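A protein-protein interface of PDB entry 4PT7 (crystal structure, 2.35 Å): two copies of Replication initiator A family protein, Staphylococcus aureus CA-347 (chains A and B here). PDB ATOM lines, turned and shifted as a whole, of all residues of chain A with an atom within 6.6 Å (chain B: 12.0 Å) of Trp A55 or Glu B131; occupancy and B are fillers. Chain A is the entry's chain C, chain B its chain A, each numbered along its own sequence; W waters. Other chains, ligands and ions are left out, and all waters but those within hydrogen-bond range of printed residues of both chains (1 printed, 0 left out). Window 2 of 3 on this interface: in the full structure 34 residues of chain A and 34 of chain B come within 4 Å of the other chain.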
ATOM      1  N   LEU A  49      11.079   0.624 -19.112  1.00  0.00           N
ATOM      2  CA  LEU A  49      11.513   0.264 -20.448  1.00  0.00           C
ATOM      3  C   LEU A  49      10.505   0.705 -21.505  1.00  0.00           C
ATOM      4  O   LEU A  49      10.897   1.087 -22.604  1.00  0.00           O
ATOM      5  CB  LEU A  49      11.756  -1.244 -20.540  1.00  0.00           C
ATOM      6  CG  LEU A  49      12.889  -1.761 -19.648  1.00  0.00           C
ATOM      7  CD1 LEU A  49      13.073  -3.257 -19.854  1.00  0.00           C
ATOM      8  CD2 LEU A  49      14.178  -1.013 -19.976  1.00  0.00           C
ATOM      9  N   SER A  50       9.212   0.663 -21.182  1.00  0.00           N
ATOM     10  CA  SER A  50       8.217   1.101 -22.158  1.00  0.00           C
ATOM     11  C   SER A  50       8.480   2.546 -22.541  1.00  0.00           C
ATOM     12  O   SER A  50       8.382   2.911 -23.708  1.00  0.00           O
ATOM     13  CB  SER A  50       6.800   0.986 -21.611  1.00  0.00           C
ATOM     14  OG  SER A  50       6.399  -0.365 -21.476  1.00  0.00           O
ATOM     15  N   ILE A  51       8.820   3.366 -21.553  1.00  0.00           N
ATOM     16  CA  ILE A  51       9.096   4.767 -21.814  1.00  0.00           C
ATOM     17  C   ILE A  51      10.262   4.894 -22.792  1.00  0.00           C
ATOM     18  O   ILE A  51      10.181   5.624 -23.777  1.00  0.00           O
ATOM     19  CB  ILE A  51       9.420   5.517 -20.508  1.00  0.00           C
ATOM     20  CG1 ILE A  51       8.156   5.605 -19.652  1.00  0.00           C
ATOM     21  CG2 ILE A  51       9.967   6.912 -20.814  1.00  0.00           C
ATOM     22  CD1 ILE A  51       8.400   6.112 -18.257  1.00  0.00           C
ATOM     23  N   LYS A  52      11.344   4.172 -22.522  1.00  0.00           N
ATOM     24  CA  LYS A  52      12.509   4.212 -23.394  1.00  0.00           C
ATOM     25  C   LYS A  52      12.180   3.726 -24.805  1.00  0.00           C
ATOM     26  O   LYS A  52      12.789   4.171 -25.774  1.00  0.00           O
ATOM     27  CB  LYS A  52      13.638   3.372 -22.798  1.00  0.00           C
ATOM     28  CG  LYS A  52      14.241   3.970 -21.543  1.00  0.00           C
ATOM     29  CD  LYS A  52      15.316   3.070 -20.961  1.00  0.00           C
ATOM     30  CE  LYS A  52      15.937   3.689 -19.721  1.00  0.00           C
ATOM     31  NZ  LYS A  52      16.923   2.767 -19.084  1.00  0.00           N
ATOM     32  N   ASN A  53      11.211   2.821 -24.915  1.00  0.00           N
ATOM     33  CA  ASN A  53      10.811   2.299 -26.217  1.00  0.00           C
ATOM     34  C   ASN A  53       9.771   3.210 -26.854  1.00  0.00           C
ATOM     35  O   ASN A  53       9.189   2.874 -27.884  1.00  0.00           O
ATOM     36  CB  ASN A  53      10.219   0.891 -26.090  1.00  0.00           C
ATOM     37  CG  ASN A  53      11.215  -0.111 -25.565  1.00  0.00           C
ATOM     38  OD1 ASN A  53      12.415   0.007 -25.808  1.00  0.00           O
ATOM     39  ND2 ASN A  53      10.722  -1.122 -24.857  1.00  0.00           N
ATOM     40  N   SER A  54       9.536   4.359 -26.227  1.00  0.00           N
ATOM     41  CA  SER A  54       8.561   5.329 -26.711  1.00  0.00           C
ATOM     42  C   SER A  54       7.154   4.744 -26.776  1.00  0.00           C
ATOM     43  O   SER A  54       6.313   5.217 -27.541  1.00  0.00           O
ATOM     44  CB  SER A  54       8.966   5.846 -28.098  1.00  0.00           C
ATOM     45  OG  SER A  54      10.294   6.339 -28.088  1.00  0.00           O
ATOM     46  N   TRP A  55       6.895   3.712 -25.978  1.00  0.00           N
ATOM     47  CA  TRP A  55       5.570   3.100 -25.956  1.00  0.00           C
ATOM     48  C   TRP A  55       4.646   3.917 -25.065  1.00  0.00           C
ATOM     49  O   TRP A  55       4.190   3.449 -24.017  1.00  0.00           O
ATOM     50  CB  TRP A  55       5.637   1.656 -25.445  1.00  0.00           C
ATOM     51  CG  TRP A  55       6.367   0.717 -26.367  1.00  0.00           C
ATOM     52  CD1 TRP A  55       6.697   0.941 -27.673  1.00  0.00           C
ATOM     53  CD2 TRP A  55       6.837  -0.600 -26.053  1.00  0.00           C
ATOM     54  NE1 TRP A  55       7.347  -0.150 -28.192  1.00  0.00           N
ATOM     55  CE2 TRP A  55       7.448  -1.113 -27.223  1.00  0.00           C
ATOM     56  CE3 TRP A  55       6.806  -1.400 -24.901  1.00  0.00           C
ATOM     57  CZ2 TRP A  55       8.023  -2.387 -27.271  1.00  0.00           C
ATOM     58  CZ3 TRP A  55       7.379  -2.666 -24.948  1.00  0.00           C
ATOM     59  CH2 TRP A  55       7.980  -3.147 -26.126  1.00  0.00           C
ATOM     60  N   VAL A  56       4.380   5.148 -25.488  1.00  0.00           N
ATOM     61  CA  VAL A  56       3.506   6.040 -24.740  1.00  0.00           C
ATOM     62  C   VAL A  56       2.315   6.423 -25.603  1.00  0.00           C
ATOM     63  O   VAL A  56       2.452   6.819 -26.758  1.00  0.00           O
ATOM     64  CB  VAL A  56       4.246   7.320 -24.297  1.00  0.00           C
ATOM     65  CG1 VAL A  56       3.311   8.216 -23.490  1.00  0.00           C
ATOM     66  CG2 VAL A  56       5.470   6.950 -23.480  1.00  0.00           C
ATOM     67  N   ASP A  57       1.141   6.287 -25.013  1.00  0.00           N
ATOM     68  CA  ASP A  57      -0.123   6.582 -25.663  1.00  0.00           C
ATOM     69  C   ASP A  57      -0.240   8.065 -26.005  1.00  0.00           C
ATOM     70  O   ASP A  57       0.547   8.883 -25.529  1.00  0.00           O
ATOM     71  CB  ASP A  57      -1.250   6.175 -24.722  1.00  0.00           C
ATOM     72  CG  ASP A  57      -2.521   5.907 -25.439  1.00  0.00           C
ATOM     73  OD1 ASP A  57      -2.448   5.535 -26.627  1.00  0.00           O
ATOM     74  OD2 ASP A  57      -3.585   6.051 -24.814  1.00  0.00           O
ATOM     75  N   ASN A  61      -0.467   7.694 -21.661  1.00  0.00           N
ATOM     76  CA  ASN A  61      -0.550   6.400 -20.991  1.00  0.00           C
ATOM     77  C   ASN A  61       0.545   5.446 -21.465  1.00  0.00           C
ATOM     78  O   ASN A  61       0.776   5.311 -22.670  1.00  0.00           O
ATOM     79  CB  ASN A  61      -1.923   5.767 -21.221  1.00  0.00           C
ATOM     80  CG  ASN A  61      -3.053   6.634 -20.704  1.00  0.00           C
ATOM     81  OD1 ASN A  61      -2.939   7.267 -19.652  1.00  0.00           O
ATOM     82  ND2 ASN A  61      -4.163   6.656 -21.437  1.00  0.00           N
ATOM     83  N   ILE A  62       1.207   4.789 -20.509  1.00  0.00           N
ATOM     84  CA  ILE A  62       2.282   3.847 -20.802  1.00  0.00           C
ATOM     85  C   ILE A  62       1.717   2.452 -21.069  1.00  0.00           C
ATOM     86  O   ILE A  62       0.897   1.949 -20.299  1.00  0.00           O
ATOM     87  CB  ILE A  62       3.287   3.774 -19.627  1.00  0.00           C
ATOM     88  CG1 ILE A  62       3.745   5.190 -19.247  1.00  0.00           C
ATOM     89  CG2 ILE A  62       4.503   2.947 -20.028  1.00  0.00           C
ATOM     90  CD1 ILE A  62       4.514   5.267 -17.931  1.00  0.00           C
ATOM     91  N   TYR A  63       2.175   1.819 -22.146  1.00  0.00           N
ATOM     92  CA  TYR A  63       1.685   0.494 -22.512  1.00  0.00           C
ATOM     93  C   TYR A  63       2.801  -0.460 -22.933  1.00  0.00           C
ATOM     94  O   TYR A  63       3.969  -0.080 -23.013  1.00  0.00           O
ATOM     95  CB  TYR A  63       0.649   0.624 -23.639  1.00  0.00           C
ATOM     96  CG  TYR A  63       1.195   1.249 -24.909  1.00  0.00           C
ATOM     97  CD1 TYR A  63       1.942   0.498 -25.818  1.00  0.00           C
ATOM     98  CD2 TYR A  63       0.997   2.606 -25.188  1.00  0.00           C
ATOM     99  CE1 TYR A  63       2.476   1.074 -26.967  1.00  0.00           C
ATOM    100  CE2 TYR A  63       1.532   3.195 -26.337  1.00  0.00           C
ATOM    101  CZ  TYR A  63       2.271   2.421 -27.222  1.00  0.00           C
ATOM    102  OH  TYR A  63       2.813   2.993 -28.355  1.00  0.00           O
ATOM    103  N   PHE A  64       2.428  -1.710 -23.184  1.00  0.00           N
ATOM    104  CA  PHE A  64       3.374  -2.740 -23.606  1.00  0.00           C
ATOM    105  C   PHE A  64       2.995  -3.266 -24.984  1.00  0.00           C
ATOM    106  O   PHE A  64       1.806  -3.377 -25.312  1.00  0.00           O
ATOM    107  CB  PHE A  64       3.378  -3.916 -22.627  1.00  0.00           C
ATOM    108  CG  PHE A  64       3.849  -3.561 -21.257  1.00  0.00           C
ATOM    109  CD1 PHE A  64       2.998  -3.683 -20.162  1.00  0.00           C
ATOM    110  CD2 PHE A  64       5.152  -3.123 -21.052  1.00  0.00           C
ATOM    111  CE1 PHE A  64       3.444  -3.370 -18.876  1.00  0.00           C
ATOM    112  CE2 PHE A  64       5.607  -2.809 -19.772  1.00  0.00           C
ATOM    113  CZ  PHE A  64       4.751  -2.934 -18.684  1.00  0.00           C
ATOM    114  N   VAL A  65       4.017  -3.589 -25.775  1.00  0.00           N
ATOM    115  CA  VAL A  65       3.833  -4.124 -27.117  1.00  0.00           C
ATOM    116  C   VAL A  65       4.678  -5.389 -27.206  1.00  0.00           C
ATOM    117  O   VAL A  65       5.297  -5.663 -28.229  1.00  0.00           O
ATOM    118  CB  VAL A  65       4.340  -3.146 -28.199  1.00  0.00           C
ATOM    119  CG1 VAL A  65       3.795  -3.553 -29.551  1.00  0.00           C
ATOM    120  CG2 VAL A  65       3.941  -1.732 -27.860  1.00  0.00           C
ATOM    121  N   TYR A  66       4.715  -6.149 -26.121  1.00  0.00           N
ATOM    122  CA  TYR A  66       5.510  -7.369 -26.088  1.00  0.00           C
ATOM    123  C   TYR A  66       4.751  -8.574 -26.649  1.00  0.00           C
ATOM    124  O   TYR A  66       3.543  -8.726 -26.432  1.00  0.00           O
ATOM    125  CB  TYR A  66       5.951  -7.662 -24.652  1.00  0.00           C
ATOM    126  CG  TYR A  66       7.013  -6.729 -24.098  1.00  0.00           C
ATOM    127  CD1 TYR A  66       6.805  -6.036 -22.903  1.00  0.00           C
ATOM    128  CD2 TYR A  66       8.248  -6.596 -24.723  1.00  0.00           C
ATOM    129  CE1 TYR A  66       7.800  -5.245 -22.344  1.00  0.00           C
ATOM    130  CE2 TYR A  66       9.259  -5.800 -24.167  1.00  0.00           C
ATOM    131  CZ  TYR A  66       9.023  -5.132 -22.976  1.00  0.00           C
ATOM    132  OH  TYR A  66      10.013  -4.363 -22.411  1.00  0.00           O
ATOM    133  N   LYS A  70       7.968 -12.951 -25.652  1.00  0.00           N
ATOM    134  CA  LYS A  70       8.706 -11.993 -24.830  1.00  0.00           C
ATOM    135  C   LYS A  70       8.191 -11.966 -23.396  1.00  0.00           C
ATOM    136  O   LYS A  70       8.965 -12.048 -22.454  1.00  0.00           O
ATOM    137  CB  LYS A  70       8.615 -10.586 -25.429  1.00  0.00           C
ATOM    138  CG  LYS A  70       9.965  -9.944 -25.705  1.00  0.00           C
ATOM    139  CD  LYS A  70      10.876  -9.964 -24.492  1.00  0.00           C
ATOM    140  CE  LYS A  70      12.205  -9.303 -24.811  1.00  0.00           C
ATOM    141  NZ  LYS A  70      13.195  -9.407 -23.713  1.00  0.00           N
ATOM    142  N   GLU B 124      21.326  -6.252 -14.603  1.00  0.00           N
ATOM    143  CA  GLU B 124      21.669  -5.107 -15.443  1.00  0.00           C
ATOM    144  C   GLU B 124      21.182  -5.319 -16.871  1.00  0.00           C
ATOM    145  O   GLU B 124      20.708  -4.390 -17.527  1.00  0.00           O
ATOM    146  CB  GLU B 124      23.185  -4.884 -15.433  1.00  0.00           C
ATOM    147  CG  GLU B 124      23.642  -3.544 -15.989  1.00  0.00           C
ATOM    148  CD  GLU B 124      22.990  -2.351 -15.285  1.00  0.00           C
ATOM    149  OE1 GLU B 124      22.648  -2.467 -14.085  1.00  0.00           O
ATOM    150  OE2 GLU B 124      22.832  -1.287 -15.930  1.00  0.00           O
ATOM    151  N   LYS B 125      21.304  -6.552 -17.346  1.00  0.00           N
ATOM    152  CA  LYS B 125      20.872  -6.900 -18.688  1.00  0.00           C
ATOM    153  C   LYS B 125      19.367  -6.683 -18.839  1.00  0.00           C
ATOM    154  O   LYS B 125      18.914  -6.117 -19.835  1.00  0.00           O
ATOM    155  CB  LYS B 125      21.213  -8.367 -18.979  1.00  0.00           C
ATOM    156  CG  LYS B 125      20.620  -8.909 -20.273  1.00  0.00           C
ATOM    157  CD  LYS B 125      20.910 -10.396 -20.434  1.00  0.00           C
ATOM    158  CE  LYS B 125      20.199 -10.985 -21.654  1.00  0.00           C
ATOM    159  NZ  LYS B 125      20.637 -10.364 -22.936  1.00  0.00           N
ATOM    160  N   GLU B 126      18.599  -7.133 -17.850  1.00  0.00           N
ATOM    161  CA  GLU B 126      17.144  -7.003 -17.893  1.00  0.00           C
ATOM    162  C   GLU B 126      16.668  -5.563 -17.742  1.00  0.00           C
ATOM    163  O   GLU B 126      15.702  -5.150 -18.388  1.00  0.00           O
ATOM    164  CB  GLU B 126      16.500  -7.877 -16.808  1.00  0.00           C
ATOM    165  CG  GLU B 126      16.946  -9.348 -16.850  1.00  0.00           C
ATOM    166  CD  GLU B 126      16.289 -10.212 -15.774  1.00  0.00           C
ATOM    167  OE1 GLU B 126      16.345  -9.843 -14.578  1.00  0.00           O
ATOM    168  OE2 GLU B 126      15.719 -11.267 -16.126  1.00  0.00           O
ATOM    169  N   GLU B 127      17.344  -4.794 -16.897  1.00  0.00           N
ATOM    170  CA  GLU B 127      16.953  -3.408 -16.680  1.00  0.00           C
ATOM    171  C   GLU B 127      17.306  -2.502 -17.858  1.00  0.00           C
ATOM    172  O   GLU B 127      16.878  -1.353 -17.917  1.00  0.00           O
ATOM    173  CB  GLU B 127      17.589  -2.871 -15.397  1.00  0.00           C
ATOM    174  CG  GLU B 127      17.016  -3.482 -14.127  1.00  0.00           C
ATOM    175  CD  GLU B 127      17.516  -2.788 -12.872  1.00  0.00           C
ATOM    176  OE1 GLU B 127      17.031  -3.118 -11.767  1.00  0.00           O
ATOM    177  OE2 GLU B 127      18.395  -1.905 -12.994  1.00  0.00           O
ATOM    178  N   ASN B 128      18.091  -3.021 -18.794  1.00  0.00           N
ATOM    179  CA  ASN B 128      18.483  -2.249 -19.971  1.00  0.00           C
ATOM    180  C   ASN B 128      18.032  -2.962 -21.234  1.00  0.00           C
ATOM    181  O   ASN B 128      18.595  -2.758 -22.309  1.00  0.00           O
ATOM    182  CB  ASN B 128      20.001  -2.061 -20.002  1.00  0.00           C
ATOM    183  CG  ASN B 128      20.507  -1.243 -18.831  1.00  0.00           C
ATOM    184  OD1 ASN B 128      20.187  -0.059 -18.694  1.00  0.00           O
ATOM    185  ND2 ASN B 128      21.297  -1.873 -17.974  1.00  0.00           N
ATOM    186  N   ASP B 129      17.013  -3.802 -21.095  1.00  0.00           N
ATOM    187  CA  ASP B 129      16.487  -4.559 -22.224  1.00  0.00           C
ATOM    188  C   ASP B 129      15.532  -3.721 -23.070  1.00  0.00           C
ATOM    189  O   ASP B 129      14.332  -4.009 -23.150  1.00  0.00           O
ATOM    190  CB  ASP B 129      15.785  -5.821 -21.719  1.00  0.00           C
ATOM    191  CG  ASP B 129      15.262  -6.694 -22.844  1.00  0.00           C
ATOM    192  OD1 ASP B 129      16.036  -6.997 -23.777  1.00  0.00           O
ATOM    193  OD2 ASP B 129      14.076  -7.085 -22.785  1.00  0.00           O
ATOM    194  N   VAL B 130      16.076  -2.683 -23.701  1.00  0.00           N
ATOM    195  CA  VAL B 130      15.285  -1.796 -24.553  1.00  0.00           C
ATOM    196  C   VAL B 130      15.035  -2.447 -25.912  1.00  0.00           C
ATOM    197  O   VAL B 130      15.857  -3.225 -26.399  1.00  0.00           O
ATOM    198  CB  VAL B 130      15.998  -0.428 -24.783  1.00  0.00           C
ATOM    199  CG1 VAL B 130      16.208   0.287 -23.451  1.00  0.00           C
ATOM    200  CG2 VAL B 130      17.335  -0.642 -25.486  1.00  0.00           C
ATOM    201  N   GLU B 131      13.893  -2.130 -26.514  1.00  0.00           N
ATOM    202  CA  GLU B 131      13.534  -2.670 -27.821  1.00  0.00           C
ATOM    203  C   GLU B 131      14.560  -2.184 -28.844  1.00  0.00           C
ATOM    204  O   GLU B 131      14.832  -0.984 -28.938  1.00  0.00           O
ATOM    205  CB  GLU B 131      12.146  -2.178 -28.231  1.00  0.00           C
ATOM    206  CG  GLU B 131      11.548  -2.930 -29.394  1.00  0.00           C
ATOM    207  CD  GLU B 131      11.012  -4.286 -28.976  1.00  0.00           C
ATOM    208  OE1 GLU B 131      11.749  -5.042 -28.303  1.00  0.00           O
ATOM    209  OE2 GLU B 131       9.849  -4.594 -29.321  1.00  0.00           O
ATOM    210  N   PRO B 132      15.141  -3.108 -29.627  1.00  0.00           N
ATOM    211  CA  PRO B 132      16.136  -2.722 -30.632  1.00  0.00           C
ATOM    212  C   PRO B 132      15.533  -1.918 -31.786  1.00  0.00           C
ATOM    213  O   PRO B 132      14.305  -2.022 -32.001  1.00  0.00           O
ATOM    214  CB  PRO B 132      16.700  -4.067 -31.086  1.00  0.00           C
ATOM    215  CG  PRO B 132      15.511  -4.970 -30.970  1.00  0.00           C
ATOM    216  CD  PRO B 132      14.922  -4.566 -29.635  1.00  0.00           C
HETATM  217  O   HOH W   1      11.933  -3.716 -24.323  1.00  0.00           O
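Of chain B, only Glu B126 (3.6 Å), Glu B127 (3.4 Å) and Asp B129 (3.6 Å) come within 4 Å of Leu A49. No residue of chain B comes within 4 Å of Ser A50. No residue of chain B comes within 4 Å of Ile A51. Of the printed residues of chain B, Lys A52 touches Val B130 (3.8 Å). Of chain B, only Val B130 and Glu B131 come within 4 Å of Asn A53. No residue of chain B comes within 4 Å of Ser A54. Of chain B, only Glu B131 (3.5 Å) comes within 4 Å of Trp A55. Val A56 touches none of the printed residues of chain B. No residue of chain B comes within 4 Å of Ile A62. No residue of chain B comes within 4 Å of Tyr A63. No residue of chain B comes within 4 Å of Phe A64. No residue of chain B comes within 4 Å of Val A65. No residue of chain B comes within 4 Å of Tyr A66. Printed residues of chain B within 4 Å of Lys A70: Asp B129. Printed residues of chain A within 4 Å of Glu B126: Leu A49 (3.6 Å). Glu B131 touches two residues of chain A. The nearest printed residue of chain B that does not touch Trp A55 is Asp B129 (7.1 Å). The nearest residue of chain A that does not touch Glu B131 is Val A65 (4.8 Å).
No position is printed for both chains. Of the 8 pairs that touch across the chains among the printed residues, none has its exchanged pair printed and touching as well.
The backbone carbonyl oxygen of Leu A49 is in hydrogen-bond range of the side-chain amide nitrogen of Asn A53, 3.2 Å away. The backbone carbonyl oxygen (O) of Ser A50 is in hydrogen-bond range of the backbone NH (N) of Trp A55, 2.8 Å away. N of Tyr A63 is in hydrogen-bond range of O of Trp A55, at 3.2 Å.
Among the printed residues, pairs that only touch across the chains: Leu A49 with Glu B127, Trp A55 with Glu B131, Leu A49 with Glu B126, Asn A53 with Val B130, Leu A49 with Asp B129 and Lys A52 with Val B130.
OD2 of Asp B129 lies within salt-bridge range of NZ of Lys A70 (2.7 Å). The side-chain amide oxygen of Asn A53 is in hydrogen-bond range of the backbone NH of Glu B131 (2.7 Å).
Hydrophobic or aromatic side chains of chain B within 4 Å of the printed part of chain A: Val B130. Of the 16 printed residues of chain A, 5 touch a printed residue of chain B. Printed residues of chain A that touch a printed residue of chain B: Leu A49, Lys A52, Asn A53, Trp A55 and Lys A70. Among the printed residues, Asp or Glu carboxylates within 4 Å of a Lys or Arg side-chain nitrogen of the other chain: Lys A70 with Asp B129.
Water W1 lies within hydrogen-bond range of the backbone carbonyl oxygen of Asp B129, the side-chain hydroxyl of Tyr A66, the side-chain amide nitrogen of Asn A53 and the backbone NH of Glu B131.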
